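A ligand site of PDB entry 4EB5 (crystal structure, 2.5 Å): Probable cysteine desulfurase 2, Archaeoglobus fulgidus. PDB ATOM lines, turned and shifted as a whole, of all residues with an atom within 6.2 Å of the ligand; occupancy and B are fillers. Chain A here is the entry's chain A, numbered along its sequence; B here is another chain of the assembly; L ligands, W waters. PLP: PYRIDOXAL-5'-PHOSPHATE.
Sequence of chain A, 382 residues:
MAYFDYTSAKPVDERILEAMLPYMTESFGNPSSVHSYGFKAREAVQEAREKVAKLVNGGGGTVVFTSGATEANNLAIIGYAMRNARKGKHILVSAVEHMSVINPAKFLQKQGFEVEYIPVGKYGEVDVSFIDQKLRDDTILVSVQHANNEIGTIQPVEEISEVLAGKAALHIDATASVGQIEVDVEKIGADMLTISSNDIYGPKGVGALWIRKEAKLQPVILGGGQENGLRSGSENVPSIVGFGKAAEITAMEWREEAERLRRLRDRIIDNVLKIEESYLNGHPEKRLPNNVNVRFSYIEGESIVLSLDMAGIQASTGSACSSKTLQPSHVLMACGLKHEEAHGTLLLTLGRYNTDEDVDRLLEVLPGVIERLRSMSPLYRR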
ATOM      1  N   THR A   7       3.834  16.474  26.192  1.00  0.00           N
ATOM      2  CA  THR A   7       4.109  15.265  25.386  1.00  0.00           C
ATOM      3  C   THR A   7       5.283  14.404  25.871  1.00  0.00           C
ATOM      4  O   THR A   7       5.264  13.199  25.635  1.00  0.00           O
ATOM      5  CB  THR A   7       4.436  15.540  23.895  1.00  0.00           C
ATOM      6  OG1 THR A   7       4.424  16.937  23.647  1.00  0.00           O
ATOM      7  CG2 THR A   7       3.452  14.867  23.021  1.00  0.00           C
ATOM      8  N   SER A   8       6.281  15.004  26.495  1.00  0.00           N
ATOM      9  CA  SER A   8       7.485  14.276  26.815  1.00  0.00           C
ATOM     10  C   SER A   8       7.522  13.715  28.217  1.00  0.00           C
ATOM     11  O   SER A   8       8.260  12.794  28.487  1.00  0.00           O
ATOM     12  CB  SER A   8       8.717  15.151  26.613  1.00  0.00           C
ATOM     13  OG  SER A   8       8.765  15.698  25.310  1.00  0.00           O
ATOM     14  N   SER A  67       6.380  -2.133  31.029  1.00  0.00           N
ATOM     15  CA  SER A  67       7.194  -1.069  31.616  1.00  0.00           C
ATOM     16  C   SER A  67       6.846   0.297  30.996  1.00  0.00           C
ATOM     17  O   SER A  67       7.405   1.322  31.398  1.00  0.00           O
ATOM     18  CB  SER A  67       8.656  -1.403  31.408  1.00  0.00           C
ATOM     19  OG  SER A  67       8.901  -1.495  30.030  1.00  0.00           O
ATOM     20  N   GLY A  68       5.936   0.304  30.030  1.00  0.00           N
ATOM     21  CA  GLY A  68       5.534   1.525  29.363  1.00  0.00           C
ATOM     22  C   GLY A  68       4.995   1.228  27.975  1.00  0.00           C
ATOM     23  O   GLY A  68       4.852   0.053  27.581  1.00  0.00           O
ATOM     24  N   ALA A  69       4.679   2.312  27.243  1.00  0.00           N
ATOM     25  CA  ALA A  69       4.125   2.241  25.891  1.00  0.00           C
ATOM     26  C   ALA A  69       5.108   1.655  24.888  1.00  0.00           C
ATOM     27  O   ALA A  69       4.720   1.035  23.913  1.00  0.00           O
ATOM     28  CB  ALA A  69       3.643   3.623  25.398  1.00  0.00           C
ATOM     29  N   THR A  70       6.391   1.874  25.151  1.00  0.00           N
ATOM     30  CA  THR A  70       7.398   1.389  24.254  1.00  0.00           C
ATOM     31  C   THR A  70       7.416  -0.150  24.212  1.00  0.00           C
ATOM     32  O   THR A  70       7.309  -0.737  23.125  1.00  0.00           O
ATOM     33  CB  THR A  70       8.748   2.050  24.560  1.00  0.00           C
ATOM     34  OG1 THR A  70       8.653   3.434  24.195  1.00  0.00           O
ATOM     35  CG2 THR A  70       9.852   1.423  23.764  1.00  0.00           C
ATOM     36  N   GLU A  71       7.477  -0.771  25.379  1.00  0.00           N
ATOM     37  CA  GLU A  71       7.433  -2.226  25.474  1.00  0.00           C
ATOM     38  C   GLU A  71       6.124  -2.859  24.954  1.00  0.00           C
ATOM     39  O   GLU A  71       6.157  -3.899  24.271  1.00  0.00           O
ATOM     40  CB  GLU A  71       7.683  -2.659  26.929  1.00  0.00           C
ATOM     41  CG  GLU A  71       7.862  -4.157  27.093  1.00  0.00           C
ATOM     42  CD  GLU A  71       7.850  -4.563  28.507  1.00  0.00           C
ATOM     43  OE1 GLU A  71       8.197  -3.745  29.380  1.00  0.00           O
ATOM     44  OE2 GLU A  71       7.470  -5.728  28.758  1.00  0.00           O
ATOM     45  N   ASN A  73       4.117  -1.569  22.687  1.00  0.00           N
ATOM     46  CA  ASN A  73       4.219  -1.464  21.234  1.00  0.00           C
ATOM     47  C   ASN A  73       5.121  -2.569  20.668  1.00  0.00           C
ATOM     48  O   ASN A  73       4.815  -3.150  19.623  1.00  0.00           O
ATOM     49  CB  ASN A  73       4.713  -0.069  20.812  1.00  0.00           C
ATOM     50  CG  ASN A  73       3.595   0.938  20.716  1.00  0.00           C
ATOM     51  OD1 ASN A  73       2.411   0.570  20.727  1.00  0.00           O
ATOM     52  ND2 ASN A  73       3.947   2.224  20.604  1.00  0.00           N
ATOM     53  N   HIS A  98       4.911   6.103  16.052  1.00  0.00           N
ATOM     54  CA  HIS A  98       6.035   6.241  16.943  1.00  0.00           C
ATOM     55  C   HIS A  98       7.210   5.328  16.571  1.00  0.00           C
ATOM     56  O   HIS A  98       7.006   4.208  16.048  1.00  0.00           O
ATOM     57  CB  HIS A  98       5.617   5.935  18.379  1.00  0.00           C
ATOM     58  CG  HIS A  98       6.578   6.494  19.356  1.00  0.00           C
ATOM     59  ND1 HIS A  98       7.504   5.706  20.001  1.00  0.00           N
ATOM     60  CD2 HIS A  98       6.852   7.774  19.706  1.00  0.00           C
ATOM     61  CE1 HIS A  98       8.276   6.480  20.754  1.00  0.00           C
ATOM     62  NE2 HIS A  98       7.909   7.741  20.584  1.00  0.00           N
ATOM     63  N   SER A 100       8.691   3.404  18.439  1.00  0.00           N
ATOM     64  CA  SER A 100       8.473   2.123  19.164  1.00  0.00           C
ATOM     65  C   SER A 100       7.519   1.152  18.458  1.00  0.00           C
ATOM     66  O   SER A 100       7.280   0.031  18.918  1.00  0.00           O
ATOM     67  CB  SER A 100       8.008   2.376  20.603  1.00  0.00           C
ATOM     68  OG  SER A 100       6.889   3.243  20.606  1.00  0.00           O
ATOM     69  N   GLN A 145      -1.784   4.401  14.671  1.00  0.00           N
ATOM     70  CA  GLN A 145      -1.993   5.168  15.895  1.00  0.00           C
ATOM     71  C   GLN A 145      -3.380   5.802  15.991  1.00  0.00           C
ATOM     72  O   GLN A 145      -4.016   6.083  14.982  1.00  0.00           O
ATOM     73  CB  GLN A 145      -0.937   6.274  16.004  1.00  0.00           C
ATOM     74  CG  GLN A 145      -0.733   7.031  14.709  1.00  0.00           C
ATOM     75  CD  GLN A 145       0.283   8.124  14.864  1.00  0.00           C
ATOM     76  OE1 GLN A 145       0.138   9.232  14.296  1.00  0.00           O
ATOM     77  NE2 GLN A 145       1.319   7.848  15.665  1.00  0.00           N
ATOM     78  N   ALA A 147      -3.841   8.799  17.295  1.00  0.00           N
ATOM     79  CA  ALA A 147      -3.561  10.204  17.024  1.00  0.00           C
ATOM     80  C   ALA A 147      -2.058  10.415  17.148  1.00  0.00           C
ATOM     81  O   ALA A 147      -1.348   9.666  17.867  1.00  0.00           O
ATOM     82  CB  ALA A 147      -4.289  11.079  18.034  1.00  0.00           C
ATOM     83  N   ASN A 148      -1.585  11.432  16.463  1.00  0.00           N
ATOM     84  CA  ASN A 148      -0.152  11.743  16.467  1.00  0.00           C
ATOM     85  C   ASN A 148       0.191  12.647  17.606  1.00  0.00           C
ATOM     86  O   ASN A 148      -0.432  13.712  17.725  1.00  0.00           O
ATOM     87  CB  ASN A 148       0.248  12.425  15.156  1.00  0.00           C
ATOM     88  CG  ASN A 148       1.713  12.323  14.920  1.00  0.00           C
ATOM     89  OD1 ASN A 148       2.487  13.272  15.184  1.00  0.00           O
ATOM     90  ND2 ASN A 148       2.149  11.126  14.468  1.00  0.00           N
ATOM     91  N   ASN A 149       1.189  12.288  18.431  1.00  0.00           N
ATOM     92  CA  ASN A 149       1.633  13.221  19.508  1.00  0.00           C
ATOM     93  C   ASN A 149       2.418  14.416  19.021  1.00  0.00           C
ATOM     94  O   ASN A 149       2.625  15.350  19.776  1.00  0.00           O
ATOM     95  CB  ASN A 149       2.392  12.556  20.675  1.00  0.00           C
ATOM     96  CG  ASN A 149       1.622  12.632  22.022  1.00  0.00           C
ATOM     97  OD1 ASN A 149       0.698  13.432  22.179  1.00  0.00           O
ATOM     98  ND2 ASN A 149       2.006  11.793  22.966  1.00  0.00           N
ATOM     99  N   ASP A 173      -2.075   2.273  18.616  1.00  0.00           N
ATOM    100  CA  ASP A 173      -1.272   2.983  19.621  1.00  0.00           C
ATOM    101  C   ASP A 173      -2.050   4.154  20.107  1.00  0.00           C
ATOM    102  O   ASP A 173      -2.236   5.083  19.322  1.00  0.00           O
ATOM    103  CB  ASP A 173       0.047   3.466  19.061  1.00  0.00           C
ATOM    104  CG  ASP A 173       0.964   4.018  20.119  1.00  0.00           C
ATOM    105  OD1 ASP A 173       0.589   4.092  21.324  1.00  0.00           O
ATOM    106  OD2 ASP A 173       2.093   4.362  19.771  1.00  0.00           O
ATOM    107  N   ALA A 174      -2.492   4.138  21.365  1.00  0.00           N
ATOM    108  CA  ALA A 174      -3.340   5.188  21.899  1.00  0.00           C
ATOM    109  C   ALA A 174      -2.671   6.059  22.990  1.00  0.00           C
ATOM    110  O   ALA A 174      -3.360   6.838  23.691  1.00  0.00           O
ATOM    111  CB  ALA A 174      -4.667   4.623  22.397  1.00  0.00           C
ATOM    112  N   THR A 175      -1.349   5.941  23.128  1.00  0.00           N
ATOM    113  CA  THR A 175      -0.561   6.806  24.012  1.00  0.00           C
ATOM    114  C   THR A 175      -0.997   8.274  23.944  1.00  0.00           C
ATOM    115  O   THR A 175      -0.964   8.971  24.960  1.00  0.00           O
ATOM    116  CB  THR A 175       0.955   6.727  23.634  1.00  0.00           C
ATOM    117  OG1 THR A 175       1.440   5.418  23.912  1.00  0.00           O
ATOM    118  CG2 THR A 175       1.815   7.714  24.400  1.00  0.00           C
ATOM    119  N   ALA A 176      -1.380   8.744  22.754  1.00  0.00           N
ATOM    120  CA  ALA A 176      -1.606  10.181  22.621  1.00  0.00           C
ATOM    121  C   ALA A 176      -3.026  10.571  23.017  1.00  0.00           C
ATOM    122  O   ALA A 176      -3.246  11.660  23.556  1.00  0.00           O
ATOM    123  CB  ALA A 176      -1.260  10.690  21.204  1.00  0.00           C
ATOM    124  N   THR A 194      -2.404   0.006  22.770  1.00  0.00           N
ATOM    125  CA  THR A 194      -1.371   0.476  23.682  1.00  0.00           C
ATOM    126  C   THR A 194      -1.853   1.668  24.532  1.00  0.00           C
ATOM    127  O   THR A 194      -2.363   2.680  23.992  1.00  0.00           O
ATOM    128  CB  THR A 194      -0.095   0.933  22.900  1.00  0.00           C
ATOM    129  OG1 THR A 194       0.450  -0.161  22.142  1.00  0.00           O
ATOM    130  CG2 THR A 194       0.942   1.505  23.905  1.00  0.00           C
ATOM    131  N   SER A 196      -0.614   4.232  28.026  1.00  0.00           N
ATOM    132  CA  SER A 196       0.534   4.692  28.744  1.00  0.00           C
ATOM    133  C   SER A 196       0.122   5.418  30.035  1.00  0.00           C
ATOM    134  O   SER A 196      -0.683   6.353  29.998  1.00  0.00           O
ATOM    135  CB  SER A 196       1.324   5.602  27.817  1.00  0.00           C
ATOM    136  OG  SER A 196       2.217   6.398  28.559  1.00  0.00           O
ATOM    137  N   ASP A 199       1.076   9.358  30.567  1.00  0.00           N
ATOM    138  CA  ASP A 199       0.238  10.229  29.713  1.00  0.00           C
ATOM    139  C   ASP A 199      -1.114  10.584  30.328  1.00  0.00           C
ATOM    140  O   ASP A 199      -1.667  11.647  30.029  1.00  0.00           O
ATOM    141  CB  ASP A 199       0.100   9.657  28.314  1.00  0.00           C
ATOM    142  CG  ASP A 199       1.391   9.876  27.474  1.00  0.00           C
ATOM    143  OD1 ASP A 199       1.299  10.439  26.344  1.00  0.00           O
ATOM    144  OD2 ASP A 199       2.506   9.533  27.958  1.00  0.00           O
ATOM    145  N   GLN B 226      17.064   5.376  23.546  1.00  0.00           N
ATOM    146  CA  GLN B 226      17.633   5.747  24.839  1.00  0.00           C
ATOM    147  C   GLN B 226      18.649   4.731  25.300  1.00  0.00           C
ATOM    148  O   GLN B 226      18.699   3.613  24.787  1.00  0.00           O
ATOM    149  CB  GLN B 226      16.540   5.915  25.886  1.00  0.00           C
ATOM    150  CG  GLN B 226      15.662   7.083  25.626  1.00  0.00           C
ATOM    151  CD  GLN B 226      14.486   6.833  24.639  1.00  0.00           C
ATOM    152  OE1 GLN B 226      14.428   5.845  23.873  1.00  0.00           O
ATOM    153  NE2 GLN B 226      13.529   7.755  24.680  1.00  0.00           N
ATOM    154  N   SER B 232      15.251   1.277  24.553  1.00  0.00           N
ATOM    155  CA  SER B 232      14.367   2.419  24.280  1.00  0.00           C
ATOM    156  C   SER B 232      13.213   2.566  25.284  1.00  0.00           C
ATOM    157  O   SER B 232      12.903   1.652  26.052  1.00  0.00           O
ATOM    158  CB  SER B 232      13.842   2.350  22.841  1.00  0.00           C
ATOM    159  OG  SER B 232      14.916   2.506  21.912  1.00  0.00           O
ATOM    160  N   GLY B 233      12.584   3.734  25.270  1.00  0.00           N
ATOM    161  CA  GLY B 233      11.556   4.078  26.252  1.00  0.00           C
ATOM    162  C   GLY B 233      11.997   5.333  26.981  1.00  0.00           C
ATOM    163  O   GLY B 233      13.184   5.461  27.290  1.00  0.00           O
ATOM    164  N   SER B 234      11.086   6.269  27.248  1.00  0.00           N
ATOM    165  CA  SER B 234      11.430   7.446  28.115  1.00  0.00           C
ATOM    166  C   SER B 234      11.920   6.968  29.475  1.00  0.00           C
ATOM    167  O   SER B 234      11.392   6.003  30.039  1.00  0.00           O
ATOM    168  CB  SER B 234      10.237   8.372  28.288  1.00  0.00           C
ATOM    169  OG  SER B 234       9.840   8.917  27.047  1.00  0.00           O
ATOM    170  N   GLU B 235      12.949   7.598  30.001  1.00  0.00           N
ATOM    171  CA  GLU B 235      13.622   7.065  31.175  1.00  0.00           C
ATOM    172  C   GLU B 235      12.760   7.313  32.451  1.00  0.00           C
ATOM    173  O   GLU B 235      12.180   8.387  32.601  1.00  0.00           O
ATOM    174  CB  GLU B 235      15.033   7.672  31.308  1.00  0.00           C
ATOM    175  CG  GLU B 235      16.033   7.313  30.184  1.00  0.00           C
ATOM    176  CD  GLU B 235      16.129   8.405  29.073  1.00  0.00           C
ATOM    177  OE1 GLU B 235      15.089   9.032  28.740  1.00  0.00           O
ATOM    178  OE2 GLU B 235      17.255   8.627  28.536  1.00  0.00           O
HETATM  179  N1  PLP L   1       3.741   5.964  21.394  1.00  0.00           N
HETATM  180  C2  PLP L   1       3.521   7.295  21.241  1.00  0.00           C
HETATM  181  C2A PLP L   1       2.387   7.758  20.342  1.00  0.00           C
HETATM  182  C3  PLP L   1       4.327   8.218  21.932  1.00  0.00           C
HETATM  183  O3  PLP L   1       4.122   9.557  21.803  1.00  0.00           O
HETATM  184  C4  PLP L   1       5.349   7.747  22.764  1.00  0.00           C
HETATM  185  C4A PLP L   1       6.198   8.697  23.471  1.00  0.00           C
HETATM  186  O4A PLP L   1       5.689   9.559  24.148  1.00  0.00           O
HETATM  187  C5  PLP L   1       5.551   6.369  22.883  1.00  0.00           C
HETATM  188  C6  PLP L   1       4.723   5.491  22.181  1.00  0.00           C
HETATM  189  C5A PLP L   1       6.615   5.760  23.787  1.00  0.00           C
HETATM  190  O4P PLP L   1       6.294   5.953  25.186  1.00  0.00           O
HETATM  191  P   PLP L   1       7.423   5.778  26.335  1.00  0.00           P
HETATM  192  O1P PLP L   1       7.659   4.295  26.348  1.00  0.00           O
HETATM  193  O2P PLP L   1       6.852   6.245  27.628  1.00  0.00           O
HETATM  194  O3P PLP L   1       8.645   6.541  25.860  1.00  0.00           O
HETATM  195  O   HOH W   1      10.473   7.198  23.579  1.00  0.00           O
HETATM  196  O   HOH W   2       8.770   3.225  28.659  1.00  0.00           O
HETATM  197  O   HOH W   3       4.699   4.959  28.392  1.00  0.00           O
HETATM  198  O   HOH W   4       5.596  11.167  19.758  1.00  0.00           O
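The side-chain amide nitrogen (ND2) of Asn 149 lies within hydrogen-bond range of an oxygen (O3) of the ligand (3.3 Å). An oxygen (O3P) of the ligand sits at hydrogen-bond distance from the backbone NH (N) of Ser 234 of chain B (2.8 Å). O1P of the ligand is in hydrogen-bond range of OG1 of Thr 70, 2.5 Å away. The side-chain hydroxyl (OG) of Ser 234 of chain B lies within hydrogen-bond range of an oxygen (O3P) of the ligand (2.9 Å). The side-chain carboxylate of Asp 173 is in hydrogen-bond range of a nitrogen (N1) of the ligand, at 2.8 Å. A nitrogen (N1) of the ligand sits at hydrogen-bond distance from the side-chain hydroxyl (OG1) of Thr 175, 3.5 Å away. An oxygen (O1P) of the ligand sits at hydrogen-bond distance from the backbone NH (N) of Thr 70 (3.0 Å).
The side-chain carboxylate (OD1) of Asp 173 sits at hydrogen-bond distance from the side-chain hydroxyl (OG1) of Thr 175 (3.0 Å). A ring nitrogen (ND1) of His 98 lies within hydrogen-bond range of the side-chain hydroxyl (OG) of Ser 100 (2.6 Å). OD2 of Asp 173 is in hydrogen-bond range of ND2 of Asn 73. The side-chain amide oxygen (OD1) of Asn 73 lies within hydrogen-bond range of the side-chain hydroxyl (OG1) of Thr 194 (2.5 Å). ND2 of Asn 73 sits at hydrogen-bond distance from OG of Ser 100 (3.1 Å). The side-chain amide oxygen of Gln 226 of chain B lies within hydrogen-bond range of the backbone NH of Gly 233 of chain B.
Merely in contact with the ligand: Thr 7, Ala 69, Asn 73, His 98, Ser 100 and Gly 233 of chain B. Of the 26 residues printed, 11 come within 4 Å of the ligand.
Water W3 lies within hydrogen-bond range of an oxygen (O2P) of the ligand (2.6 Å), the side-chain hydroxyl (OG) of Ser 196 (2.9 Å) and the backbone NH (N) of Ala 69 (2.9 Å). Water W1 bridges O3P of the ligand (3.0 Å) and NE2 of Gln 226 of chain B (3.3 Å).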
